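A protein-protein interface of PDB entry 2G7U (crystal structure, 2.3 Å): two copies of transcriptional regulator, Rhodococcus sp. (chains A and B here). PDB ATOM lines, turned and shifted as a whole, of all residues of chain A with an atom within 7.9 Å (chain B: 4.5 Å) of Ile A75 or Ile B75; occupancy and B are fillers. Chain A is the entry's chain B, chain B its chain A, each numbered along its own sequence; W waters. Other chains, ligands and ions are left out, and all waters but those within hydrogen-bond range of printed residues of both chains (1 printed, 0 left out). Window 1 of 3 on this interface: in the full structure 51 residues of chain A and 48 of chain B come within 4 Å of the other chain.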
ATOM      1  N   GLY A  16      12.788  -6.423 -35.340  1.00  0.00           N
ATOM      2  CA  GLY A  16      12.779  -6.369 -33.893  1.00  0.00           C
ATOM      3  C   GLY A  16      12.668  -4.936 -33.439  1.00  0.00           C
ATOM      4  O   GLY A  16      11.837  -4.622 -32.578  1.00  0.00           O
ATOM      5  N   PHE A  17      13.491  -4.054 -34.011  1.00  0.00           N
ATOM      6  CA  PHE A  17      13.423  -2.636 -33.638  1.00  0.00           C
ATOM      7  C   PHE A  17      12.102  -2.000 -34.041  1.00  0.00           C
ATOM      8  O   PHE A  17      11.528  -1.218 -33.275  1.00  0.00           O
ATOM      9  CB  PHE A  17      14.605  -1.847 -34.179  1.00  0.00           C
ATOM     10  CG  PHE A  17      15.887  -2.139 -33.452  1.00  0.00           C
ATOM     11  CD1 PHE A  17      16.932  -2.795 -34.089  1.00  0.00           C
ATOM     12  CD2 PHE A  17      16.035  -1.791 -32.116  1.00  0.00           C
ATOM     13  CE1 PHE A  17      18.113  -3.091 -33.403  1.00  0.00           C
ATOM     14  CE2 PHE A  17      17.211  -2.081 -31.426  1.00  0.00           C
ATOM     15  CZ  PHE A  17      18.251  -2.728 -32.070  1.00  0.00           C
ATOM     16  N   LEU A  20       9.567  -2.713 -31.371  1.00  0.00           N
ATOM     17  CA  LEU A  20       9.834  -1.850 -30.216  1.00  0.00           C
ATOM     18  C   LEU A  20       9.399  -0.409 -30.454  1.00  0.00           C
ATOM     19  O   LEU A  20       8.799   0.224 -29.588  1.00  0.00           O
ATOM     20  CB  LEU A  20      11.321  -1.879 -29.833  1.00  0.00           C
ATOM     21  CG  LEU A  20      11.869  -3.168 -29.209  1.00  0.00           C
ATOM     22  CD1 LEU A  20      13.382  -3.066 -29.011  1.00  0.00           C
ATOM     23  CD2 LEU A  20      11.166  -3.445 -27.882  1.00  0.00           C
ATOM     24  N   LEU A  21       9.702   0.102 -31.641  1.00  0.00           N
ATOM     25  CA  LEU A  21       9.373   1.485 -31.996  1.00  0.00           C
ATOM     26  C   LEU A  21       7.900   1.677 -32.333  1.00  0.00           C
ATOM     27  O   LEU A  21       7.435   2.812 -32.419  1.00  0.00           O
ATOM     28  CB  LEU A  21      10.264   1.970 -33.154  1.00  0.00           C
ATOM     29  CG  LEU A  21      11.774   2.020 -32.849  1.00  0.00           C
ATOM     30  CD1 LEU A  21      12.538   2.230 -34.132  1.00  0.00           C
ATOM     31  CD2 LEU A  21      12.127   3.105 -31.839  1.00  0.00           C
ATOM     32  N   PHE A  23       5.546   0.981 -30.382  1.00  0.00           N
ATOM     33  CA  PHE A  23       4.902   1.297 -29.126  1.00  0.00           C
ATOM     34  C   PHE A  23       4.803   2.824 -28.968  1.00  0.00           C
ATOM     35  O   PHE A  23       5.701   3.568 -29.365  1.00  0.00           O
ATOM     36  CB  PHE A  23       5.701   0.706 -27.954  1.00  0.00           C
ATOM     37  CG  PHE A  23       5.436  -0.761 -27.684  1.00  0.00           C
ATOM     38  CD1 PHE A  23       6.219  -1.753 -28.287  1.00  0.00           C
ATOM     39  CD2 PHE A  23       4.430  -1.152 -26.789  1.00  0.00           C
ATOM     40  CE1 PHE A  23       5.991  -3.122 -28.029  1.00  0.00           C
ATOM     41  CE2 PHE A  23       4.185  -2.508 -26.516  1.00  0.00           C
ATOM     42  CZ  PHE A  23       4.968  -3.496 -27.127  1.00  0.00           C
ATOM     43  N   TYR A  58      12.412  -7.584 -22.707  1.00  0.00           N
ATOM     44  CA  TYR A  58      12.084  -6.235 -23.189  1.00  0.00           C
ATOM     45  C   TYR A  58      10.590  -5.912 -23.230  1.00  0.00           C
ATOM     46  O   TYR A  58      10.202  -4.737 -23.171  1.00  0.00           O
ATOM     47  CB  TYR A  58      12.709  -5.982 -24.562  1.00  0.00           C
ATOM     48  CG  TYR A  58      14.197  -5.946 -24.471  1.00  0.00           C
ATOM     49  CD1 TYR A  58      14.967  -6.995 -24.969  1.00  0.00           C
ATOM     50  CD2 TYR A  58      14.846  -4.887 -23.812  1.00  0.00           C
ATOM     51  CE1 TYR A  58      16.360  -6.979 -24.854  1.00  0.00           C
ATOM     52  CE2 TYR A  58      16.236  -4.860 -23.690  1.00  0.00           C
ATOM     53  CZ  TYR A  58      16.987  -5.909 -24.214  1.00  0.00           C
ATOM     54  OH  TYR A  58      18.356  -5.877 -24.085  1.00  0.00           O
ATOM     55  N   LEU A  68       6.027  -2.661 -22.973  1.00  0.00           N
ATOM     56  CA  LEU A  68       7.476  -2.553 -22.805  1.00  0.00           C
ATOM     57  C   LEU A  68       7.820  -2.761 -21.318  1.00  0.00           C
ATOM     58  O   LEU A  68       6.945  -2.653 -20.454  1.00  0.00           O
ATOM     59  CB  LEU A  68       7.953  -1.194 -23.316  1.00  0.00           C
ATOM     60  CG  LEU A  68       7.928  -0.971 -24.831  1.00  0.00           C
ATOM     61  CD1 LEU A  68       8.372   0.411 -25.246  1.00  0.00           C
ATOM     62  CD2 LEU A  68       8.796  -1.991 -25.541  1.00  0.00           C
ATOM     63  N   PRO A  70      11.041  -1.864 -18.222  1.00  0.00           N
ATOM     64  CA  PRO A  70      12.121  -0.889 -18.014  1.00  0.00           C
ATOM     65  C   PRO A  70      13.430  -1.328 -18.676  1.00  0.00           C
ATOM     66  O   PRO A  70      14.302  -0.495 -18.948  1.00  0.00           O
ATOM     67  CB  PRO A  70      12.270  -0.848 -16.484  1.00  0.00           C
ATOM     68  CG  PRO A  70      11.014  -1.447 -15.943  1.00  0.00           C
ATOM     69  CD  PRO A  70      10.556  -2.430 -16.943  1.00  0.00           C
ATOM     70  N   ARG A  71      13.546  -2.625 -18.959  1.00  0.00           N
ATOM     71  CA  ARG A  71      14.739  -3.173 -19.615  1.00  0.00           C
ATOM     72  C   ARG A  71      14.920  -2.559 -20.991  1.00  0.00           C
ATOM     73  O   ARG A  71      15.972  -2.677 -21.586  1.00  0.00           O
ATOM     74  CB  ARG A  71      14.670  -4.698 -19.694  1.00  0.00           C
ATOM     75  CG  ARG A  71      16.024  -5.392 -19.620  1.00  0.00           C
ATOM     76  CD  ARG A  71      15.890  -6.916 -19.468  1.00  0.00           C
ATOM     77  NE  ARG A  71      15.828  -7.363 -18.067  1.00  0.00           N
ATOM     78  CZ  ARG A  71      14.713  -7.684 -17.405  1.00  0.00           C
ATOM     79  NH1 ARG A  71      13.519  -7.612 -17.990  1.00  0.00           N
ATOM     80  NH2 ARG A  71      14.788  -8.074 -16.139  1.00  0.00           N
ATOM     81  N   VAL A  72      13.904  -1.854 -21.479  1.00  0.00           N
ATOM     82  CA  VAL A  72      13.991  -1.194 -22.773  1.00  0.00           C
ATOM     83  C   VAL A  72      14.820   0.092 -22.698  1.00  0.00           C
ATOM     84  O   VAL A  72      15.361   0.537 -23.698  1.00  0.00           O
ATOM     85  CB  VAL A  72      12.568  -0.961 -23.406  1.00  0.00           C
ATOM     86  CG1 VAL A  72      11.914   0.328 -22.900  1.00  0.00           C
ATOM     87  CG2 VAL A  72      12.651  -0.948 -24.918  1.00  0.00           C
ATOM     88  N   LEU A  73      14.913   0.688 -21.510  1.00  0.00           N
ATOM     89  CA  LEU A  73      15.724   1.899 -21.299  1.00  0.00           C
ATOM     90  C   LEU A  73      17.212   1.554 -21.104  1.00  0.00           C
ATOM     91  O   LEU A  73      18.083   2.421 -21.182  1.00  0.00           O
ATOM     92  CB  LEU A  73      15.211   2.677 -20.084  1.00  0.00           C
ATOM     93  CG  LEU A  73      13.728   3.049 -19.984  1.00  0.00           C
ATOM     94  CD1 LEU A  73      13.429   3.534 -18.571  1.00  0.00           C
ATOM     95  CD2 LEU A  73      13.373   4.121 -20.986  1.00  0.00           C
ATOM     96  N   SER A  74      17.477   0.268 -20.883  1.00  0.00           N
ATOM     97  CA  SER A  74      18.793  -0.227 -20.500  1.00  0.00           C
ATOM     98  C   SER A  74      19.725  -0.138 -21.685  1.00  0.00           C
ATOM     99  O   SER A  74      20.884   0.242 -21.548  1.00  0.00           O
ATOM    100  CB  SER A  74      18.711  -1.679 -20.006  1.00  0.00           C
ATOM    101  OG  SER A  74      19.111  -2.580 -21.030  1.00  0.00           O
ATOM    102  N   ILE A  75      19.213  -0.474 -22.853  1.00  0.00           N
ATOM    103  CA  ILE A  75      20.019  -0.361 -24.043  1.00  0.00           C
ATOM    104  C   ILE A  75      20.467   1.080 -24.315  1.00  0.00           C
ATOM    105  O   ILE A  75      21.634   1.315 -24.629  1.00  0.00           O
ATOM    106  CB  ILE A  75      19.347  -1.040 -25.268  1.00  0.00           C
ATOM    107  CG1 ILE A  75      20.026  -0.590 -26.576  1.00  0.00           C
ATOM    108  CG2 ILE A  75      17.817  -0.847 -25.229  1.00  0.00           C
ATOM    109  CD1 ILE A  75      19.096  -0.523 -27.766  1.00  0.00           C
ATOM    110  N   GLY A  76      19.547   2.037 -24.174  1.00  0.00           N
ATOM    111  CA  GLY A  76      19.873   3.458 -24.267  1.00  0.00           C
ATOM    112  C   GLY A  76      20.944   3.882 -23.284  1.00  0.00           C
ATOM    113  O   GLY A  76      21.819   4.668 -23.621  1.00  0.00           O
ATOM    114  N   GLN A  77      20.885   3.340 -22.069  1.00  0.00           N
ATOM    115  CA  GLN A  77      21.838   3.654 -20.997  1.00  0.00           C
ATOM    116  C   GLN A  77      23.261   3.238 -21.322  1.00  0.00           C
ATOM    117  O   GLN A  77      24.198   3.817 -20.784  1.00  0.00           O
ATOM    118  CB  GLN A  77      21.438   2.955 -19.703  1.00  0.00           C
ATOM    119  CG  GLN A  77      20.250   3.548 -18.965  1.00  0.00           C
ATOM    120  CD  GLN A  77      19.741   2.596 -17.884  1.00  0.00           C
ATOM    121  OE1 GLN A  77      20.531   1.830 -17.294  1.00  0.00           O
ATOM    122  NE2 GLN A  77      18.417   2.630 -17.620  1.00  0.00           N
ATOM    123  N   HIS A  78      23.415   2.215 -22.165  1.00  0.00           N
ATOM    124  CA  HIS A  78      24.726   1.830 -22.707  1.00  0.00           C
ATOM    125  C   HIS A  78      25.381   2.891 -23.601  1.00  0.00           C
ATOM    126  O   HIS A  78      26.611   3.052 -23.564  1.00  0.00           O
ATOM    127  CB  HIS A  78      24.637   0.484 -23.448  1.00  0.00           C
ATOM    128  CG  HIS A  78      24.573  -0.695 -22.527  1.00  0.00           C
ATOM    129  ND1 HIS A  78      25.572  -1.642 -22.458  1.00  0.00           N
ATOM    130  CD2 HIS A  78      23.649  -1.057 -21.606  1.00  0.00           C
ATOM    131  CE1 HIS A  78      25.254  -2.550 -21.549  1.00  0.00           C
ATOM    132  NE2 HIS A  78      24.094  -2.216 -21.016  1.00  0.00           N
ATOM    133  N   TYR A  79      24.593   3.606 -24.414  1.00  0.00           N
ATOM    134  CA  TYR A  79      25.145   4.762 -25.130  1.00  0.00           C
ATOM    135  C   TYR A  79      25.797   5.762 -24.146  1.00  0.00           C
ATOM    136  O   TYR A  79      26.947   6.134 -24.310  1.00  0.00           O
ATOM    137  CB  TYR A  79      24.106   5.466 -26.054  1.00  0.00           C
ATOM    138  CG  TYR A  79      24.637   6.805 -26.544  1.00  0.00           C
ATOM    139  CD1 TYR A  79      25.479   6.877 -27.646  1.00  0.00           C
ATOM    140  CD2 TYR A  79      24.357   7.987 -25.843  1.00  0.00           C
ATOM    141  CE1 TYR A  79      26.012   8.097 -28.058  1.00  0.00           C
ATOM    142  CE2 TYR A  79      24.895   9.220 -26.239  1.00  0.00           C
ATOM    143  CZ  TYR A  79      25.721   9.263 -27.335  1.00  0.00           C
ATOM    144  OH  TYR A  79      26.229  10.482 -27.749  1.00  0.00           O
ATOM    145  N   SER A  80      25.054   6.143 -23.114  1.00  0.00           N
ATOM    146  CA  SER A  80      25.497   7.076 -22.067  1.00  0.00           C
ATOM    147  C   SER A  80      26.690   6.575 -21.266  1.00  0.00           C
ATOM    148  O   SER A  80      27.595   7.339 -20.954  1.00  0.00           O
ATOM    149  CB  SER A  80      24.353   7.349 -21.070  1.00  0.00           C
ATOM    150  OG  SER A  80      23.125   7.642 -21.735  1.00  0.00           O
ATOM    151  N   GLU A  81      26.667   5.301 -20.902  1.00  0.00           N
ATOM    152  CA  GLU A  81      27.728   4.710 -20.101  1.00  0.00           C
ATOM    153  C   GLU A  81      29.052   4.709 -20.838  1.00  0.00           C
ATOM    154  O   GLU A  81      30.096   4.858 -20.218  1.00  0.00           O
ATOM    155  CB  GLU A  81      27.380   3.276 -19.749  1.00  0.00           C
ATOM    156  CG  GLU A  81      26.612   3.143 -18.465  1.00  0.00           C
ATOM    157  CD  GLU A  81      25.921   1.799 -18.350  1.00  0.00           C
ATOM    158  OE1 GLU A  81      26.387   0.817 -18.986  1.00  0.00           O
ATOM    159  OE2 GLU A  81      24.904   1.733 -17.624  1.00  0.00           O
ATOM    160  N   SER A  82      28.989   4.525 -22.159  1.00  0.00           N
ATOM    161  CA  SER A  82      30.159   4.471 -23.033  1.00  0.00           C
ATOM    162  C   SER A  82      30.520   5.831 -23.653  1.00  0.00           C
ATOM    163  O   SER A  82      31.428   5.926 -24.500  1.00  0.00           O
ATOM    164  CB  SER A  82      29.909   3.450 -24.140  1.00  0.00           C
ATOM    165  OG  SER A  82      28.859   3.875 -24.998  1.00  0.00           O
ATOM    166  N   VAL A 132      15.006  12.705 -23.034  1.00  0.00           N
ATOM    167  CA  VAL A 132      16.271  12.161 -23.543  1.00  0.00           C
ATOM    168  C   VAL A 132      15.886  11.181 -24.653  1.00  0.00           C
ATOM    169  O   VAL A 132      14.965  10.373 -24.481  1.00  0.00           O
ATOM    170  CB  VAL A 132      17.104  11.453 -22.412  1.00  0.00           C
ATOM    171  CG1 VAL A 132      18.138  10.479 -22.962  1.00  0.00           C
ATOM    172  CG2 VAL A 132      17.784  12.473 -21.516  1.00  0.00           C
ATOM    173  N   GLY A 133      16.572  11.277 -25.787  1.00  0.00           N
ATOM    174  CA  GLY A 133      16.265  10.447 -26.950  1.00  0.00           C
ATOM    175  C   GLY A 133      15.354  11.126 -27.965  1.00  0.00           C
ATOM    176  O   GLY A 133      15.125  10.594 -29.036  1.00  0.00           O
ATOM    177  N   THR A 134      14.816  12.295 -27.624  1.00  0.00           N
ATOM    178  CA  THR A 134      14.021  13.110 -28.570  1.00  0.00           C
ATOM    179  C   THR A 134      14.893  13.538 -29.733  1.00  0.00           C
ATOM    180  O   THR A 134      16.073  13.866 -29.555  1.00  0.00           O
ATOM    181  CB  THR A 134      13.378  14.347 -27.871  1.00  0.00           C
ATOM    182  OG1 THR A 134      12.569  13.876 -26.797  1.00  0.00           O
ATOM    183  CG2 THR A 134      12.493  15.133 -28.810  1.00  0.00           C
ATOM    184  N   ARG A 135      14.306  13.517 -30.919  1.00  0.00           N
ATOM    185  CA  ARG A 135      15.017  13.815 -32.141  1.00  0.00           C
ATOM    186  C   ARG A 135      14.388  15.039 -32.770  1.00  0.00           C
ATOM    187  O   ARG A 135      13.170  15.149 -32.828  1.00  0.00           O
ATOM    188  CB  ARG A 135      14.900  12.638 -33.111  1.00  0.00           C
ATOM    189  CG  ARG A 135      15.164  11.283 -32.483  1.00  0.00           C
ATOM    190  CD  ARG A 135      14.920  10.174 -33.494  1.00  0.00           C
ATOM    191  NE  ARG A 135      15.868  10.244 -34.607  1.00  0.00           N
ATOM    192  CZ  ARG A 135      17.100   9.740 -34.596  1.00  0.00           C
ATOM    193  NH1 ARG A 135      17.581   9.120 -33.517  1.00  0.00           N
ATOM    194  NH2 ARG A 135      17.862   9.872 -35.668  1.00  0.00           N
ATOM    195  N   LEU B  20      24.785  -5.146 -28.915  1.00  0.00           N
ATOM    196  CA  LEU B  20      24.524  -3.781 -28.473  1.00  0.00           C
ATOM    197  C   LEU B  20      24.882  -3.590 -27.021  1.00  0.00           C
ATOM    198  O   LEU B  20      25.352  -2.517 -26.631  1.00  0.00           O
ATOM    199  CB  LEU B  20      23.042  -3.399 -28.635  1.00  0.00           C
ATOM    200  CG  LEU B  20      22.523  -3.023 -30.030  1.00  0.00           C
ATOM    201  CD1 LEU B  20      21.040  -2.744 -29.934  1.00  0.00           C
ATOM    202  CD2 LEU B  20      23.263  -1.792 -30.598  1.00  0.00           C
ATOM    203  N   LEU B  21      24.614  -4.620 -26.216  1.00  0.00           N
ATOM    204  CA  LEU B  21      24.825  -4.561 -24.779  1.00  0.00           C
ATOM    205  C   LEU B  21      26.277  -4.759 -24.400  1.00  0.00           C
ATOM    206  O   LEU B  21      26.657  -4.498 -23.261  1.00  0.00           O
ATOM    207  CB  LEU B  21      23.941  -5.592 -24.056  1.00  0.00           C
ATOM    208  CG  LEU B  21      22.421  -5.330 -24.104  1.00  0.00           C
ATOM    209  CD1 LEU B  21      21.688  -6.464 -23.415  1.00  0.00           C
ATOM    210  CD2 LEU B  21      22.021  -4.005 -23.455  1.00  0.00           C
ATOM    211  N   TYR B  58      22.639   2.245 -35.740  1.00  0.00           N
ATOM    212  CA  TYR B  58      22.786   2.042 -34.287  1.00  0.00           C
ATOM    213  C   TYR B  58      24.221   1.990 -33.821  1.00  0.00           C
ATOM    214  O   TYR B  58      24.493   2.304 -32.675  1.00  0.00           O
ATOM    215  CB  TYR B  58      22.014   0.809 -33.779  1.00  0.00           C
ATOM    216  CG  TYR B  58      20.511   0.996 -33.786  1.00  0.00           C
ATOM    217  CD1 TYR B  58      19.740   0.504 -34.831  1.00  0.00           C
ATOM    218  CD2 TYR B  58      19.866   1.700 -32.769  1.00  0.00           C
ATOM    219  CE1 TYR B  58      18.360   0.703 -34.861  1.00  0.00           C
ATOM    220  CE2 TYR B  58      18.504   1.894 -32.789  1.00  0.00           C
ATOM    221  CZ  TYR B  58      17.754   1.385 -33.831  1.00  0.00           C
ATOM    222  OH  TYR B  58      16.386   1.556 -33.853  1.00  0.00           O
ATOM    223  N   ARG B  71      21.340   6.831 -31.596  1.00  0.00           N
ATOM    224  CA  ARG B  71      20.053   6.292 -32.026  1.00  0.00           C
ATOM    225  C   ARG B  71      19.361   5.373 -31.046  1.00  0.00           C
ATOM    226  O   ARG B  71      18.122   5.360 -30.978  1.00  0.00           O
ATOM    227  CB  ARG B  71      20.162   5.601 -33.388  1.00  0.00           C
ATOM    228  CG  ARG B  71      18.774   5.316 -34.016  1.00  0.00           C
ATOM    229  CD  ARG B  71      18.825   5.157 -35.517  1.00  0.00           C
ATOM    230  NE  ARG B  71      19.477   6.323 -36.087  1.00  0.00           N
ATOM    231  CZ  ARG B  71      19.371   6.706 -37.349  1.00  0.00           C
ATOM    232  NH1 ARG B  71      18.634   6.006 -38.201  1.00  0.00           N
ATOM    233  NH2 ARG B  71      20.023   7.784 -37.756  1.00  0.00           N
ATOM    234  N   VAL B  72      20.125   4.601 -30.289  1.00  0.00           N
ATOM    235  CA  VAL B  72      19.523   3.742 -29.249  1.00  0.00           C
ATOM    236  C   VAL B  72      18.759   4.513 -28.178  1.00  0.00           C
ATOM    237  O   VAL B  72      17.928   3.935 -27.486  1.00  0.00           O
ATOM    238  CB  VAL B  72      20.571   2.831 -28.527  1.00  0.00           C
ATOM    239  CG1 VAL B  72      21.124   1.834 -29.491  1.00  0.00           C
ATOM    240  CG2 VAL B  72      21.742   3.667 -27.885  1.00  0.00           C
ATOM    241  N   LEU B  73      19.060   5.803 -28.035  1.00  0.00           N
ATOM    242  CA  LEU B  73      18.429   6.667 -27.005  1.00  0.00           C
ATOM    243  C   LEU B  73      16.955   6.871 -27.314  1.00  0.00           C
ATOM    244  O   LEU B  73      16.118   7.063 -26.415  1.00  0.00           O
ATOM    245  CB  LEU B  73      19.128   8.046 -26.926  1.00  0.00           C
ATOM    246  CG  LEU B  73      20.459   8.125 -26.152  1.00  0.00           C
ATOM    247  CD1 LEU B  73      21.157   9.432 -26.388  1.00  0.00           C
ATOM    248  CD2 LEU B  73      20.242   7.920 -24.640  1.00  0.00           C
ATOM    249  N   SER B  74      16.643   6.821 -28.600  1.00  0.00           N
ATOM    250  CA  SER B  74      15.294   7.074 -29.065  1.00  0.00           C
ATOM    251  C   SER B  74      14.319   5.912 -28.799  1.00  0.00           C
ATOM    252  O   SER B  74      13.104   6.116 -28.800  1.00  0.00           O
ATOM    253  CB  SER B  74      15.339   7.486 -30.531  1.00  0.00           C
ATOM    254  OG  SER B  74      16.289   8.549 -30.689  1.00  0.00           O
ATOM    255  N   ILE B  75      14.843   4.713 -28.539  1.00  0.00           N
ATOM    256  CA  ILE B  75      14.000   3.577 -28.128  1.00  0.00           C
ATOM    257  C   ILE B  75      13.234   3.814 -26.813  1.00  0.00           C
ATOM    258  O   ILE B  75      12.023   3.601 -26.741  1.00  0.00           O
ATOM    259  CB  ILE B  75      14.816   2.267 -28.040  1.00  0.00           C
ATOM    260  CG1 ILE B  75      15.615   2.076 -29.332  1.00  0.00           C
ATOM    261  CG2 ILE B  75      13.896   1.078 -27.765  1.00  0.00           C
ATOM    262  CD1 ILE B  75      16.351   0.782 -29.414  1.00  0.00           C
ATOM    263  N   GLY B  76      13.933   4.250 -25.772  1.00  0.00           N
ATOM    264  CA  GLY B  76      13.276   4.517 -24.490  1.00  0.00           C
ATOM    265  C   GLY B  76      12.112   5.507 -24.503  1.00  0.00           C
ATOM    266  O   GLY B  76      11.223   5.423 -23.656  1.00  0.00           O
ATOM    267  N   GLN B  77      12.093   6.442 -25.451  1.00  0.00           N
ATOM    268  CA  GLN B  77      11.011   7.419 -25.502  1.00  0.00           C
ATOM    269  C   GLN B  77       9.639   6.857 -25.963  1.00  0.00           C
ATOM    270  O   GLN B  77       8.614   7.557 -25.896  1.00  0.00           O
ATOM    271  CB  GLN B  77      11.433   8.648 -26.305  1.00  0.00           C
ATOM    272  CG  GLN B  77      11.215   8.544 -27.792  1.00  0.00           C
ATOM    273  CD  GLN B  77      12.038   9.561 -28.509  1.00  0.00           C
ATOM    274  OE1 GLN B  77      12.569  10.472 -27.864  1.00  0.00           O
ATOM    275  NE2 GLN B  77      12.174   9.421 -29.846  1.00  0.00           N
ATOM    276  N   HIS B  78       9.624   5.596 -26.394  1.00  0.00           N
ATOM    277  CA  HIS B  78       8.389   4.901 -26.722  1.00  0.00           C
ATOM    278  C   HIS B  78       7.757   4.264 -25.466  1.00  0.00           C
ATOM    279  O   HIS B  78       6.779   3.493 -25.558  1.00  0.00           O
ATOM    280  CB  HIS B  78       8.644   3.868 -27.837  1.00  0.00           C
ATOM    281  CG  HIS B  78       9.011   4.491 -29.152  1.00  0.00           C
ATOM    282  ND1 HIS B  78       8.143   4.544 -30.223  1.00  0.00           N
ATOM    283  CD2 HIS B  78      10.143   5.118 -29.555  1.00  0.00           C
ATOM    284  CE1 HIS B  78       8.731   5.162 -31.235  1.00  0.00           C
ATOM    285  NE2 HIS B  78       9.945   5.520 -30.857  1.00  0.00           N
HETATM  286  O   HOH W   1      11.771  12.210 -31.515  1.00  0.00           O
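Of the 24 printed residues of chain A, 15 touch a printed residue of chain B.
Of the 11 printed residues of chain B, 11 touch a printed residue of chain A.
Hydrophobic or aromatic side chains of chain B within 4 Å of the printed part of chain A: Leu B20, Leu B21, Tyr B58, Val B72, Leu B73, Ile B75 and His B78.
The backbone carbonyl oxygen (O) of Gly A133 sits at hydrogen-bond distance from the side-chain hydroxyl (OG) of Ser B74.
The side-chain hydroxyl (OG) of Ser B74 lies within hydrogen-bond range of the guanidinium group (NH1) of Arg A135 (3.2 Å).
A ring nitrogen (ND1) of His A78 lies close to the backbone carbonyl oxygen of Leu B21 (3.2 Å).
A ring nitrogen (ND1) of His B78 is in hydrogen-bond range of the backbone carbonyl oxygen (O) of Leu A21 (2.9 Å).
The side-chain amide oxygen (OE1) of Gln B77 lies within hydrogen-bond range of the backbone NH (N) of Thr A134, at 2.9 Å.
A ring nitrogen (ND1) of His B78 sits at hydrogen-bond distance from the backbone carbonyl oxygen of Phe A23.
O of Gly A133 lies close to OE1 of Gln B77, at 2.8 Å.
Water W1 lies within hydrogen-bond range of the backbone NH of Arg A135 and the side-chain amide nitrogen of Gln B77.
Ile A75 touches three residues of chain B.
Printed residues of chain A within 4 Å of Ile B75: Phe A17, Val A72 and Ile A75.
Gly B76 touches one residue of chain A.
Printed residues of chain B within 4 Å of His A78: Leu B21 (2.9 Å).
Printed residues of chain B within 4 Å of Thr A134: Gln B77.
Of the printed residues of chain B, Val A72 touches Ile B75.
Of the printed residues of chain B, Leu A68 touches His B78 (3.5 Å).
Ser A82 touches none of the printed residues of chain B.
The nearest residue of chain B that does not touch Ile A75 is Leu B21 (4.2 Å).
O of His A78 lies within hydrogen-bond range of OG of Ser A82 (2.8 Å).
The side-chain hydroxyl (OG) of Ser A82 sits at hydrogen-bond distance from the backbone carbonyl oxygen (O) of Tyr A79 (3.0 Å).
Leu A21 touches His B78, and with the chains exchanged His A78 touches Leu B21.
Ile A75 touches Leu B20, but with the chains exchanged Leu A20 does not touch Ile B75 (4.4 Å).
Ile B75 touches its own counterpart, Ile A75.
Gly A76 touches Val B72, but with the chains exchanged Val A72 does not touch Gly B76 (4.5 Å).
Positions printed for both chains: 20, 21, 58, 71, 72, 73, 74, 75, 76, 77 and 78.
Of the 25 pairs that touch across the chains among the printed residues, 9 have their exchanged pair printed and touching as well.
CD1 of Leu B20 touches CZ of Phe A17 (3.5 Å).
Phe A17 touches Ile B75 (CE2 to CD1, 3.6 Å).
Leu A21 touches Tyr B58 (CD1 to OH, 3.9 Å).
Tyr A58 touches Leu B21.
CD1 of Leu A68 touches O of His B78, at 3.5 Å.
Ile A75 touches Leu B20 (CD1 to CD1, 3.7 Å).
Val B72 touches Gly A76 (O to CA, 3.8 Å).
Leu B73 touches Gly A76.
Tyr A79 touches Val B72.
Arg A135 touches Arg B71.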
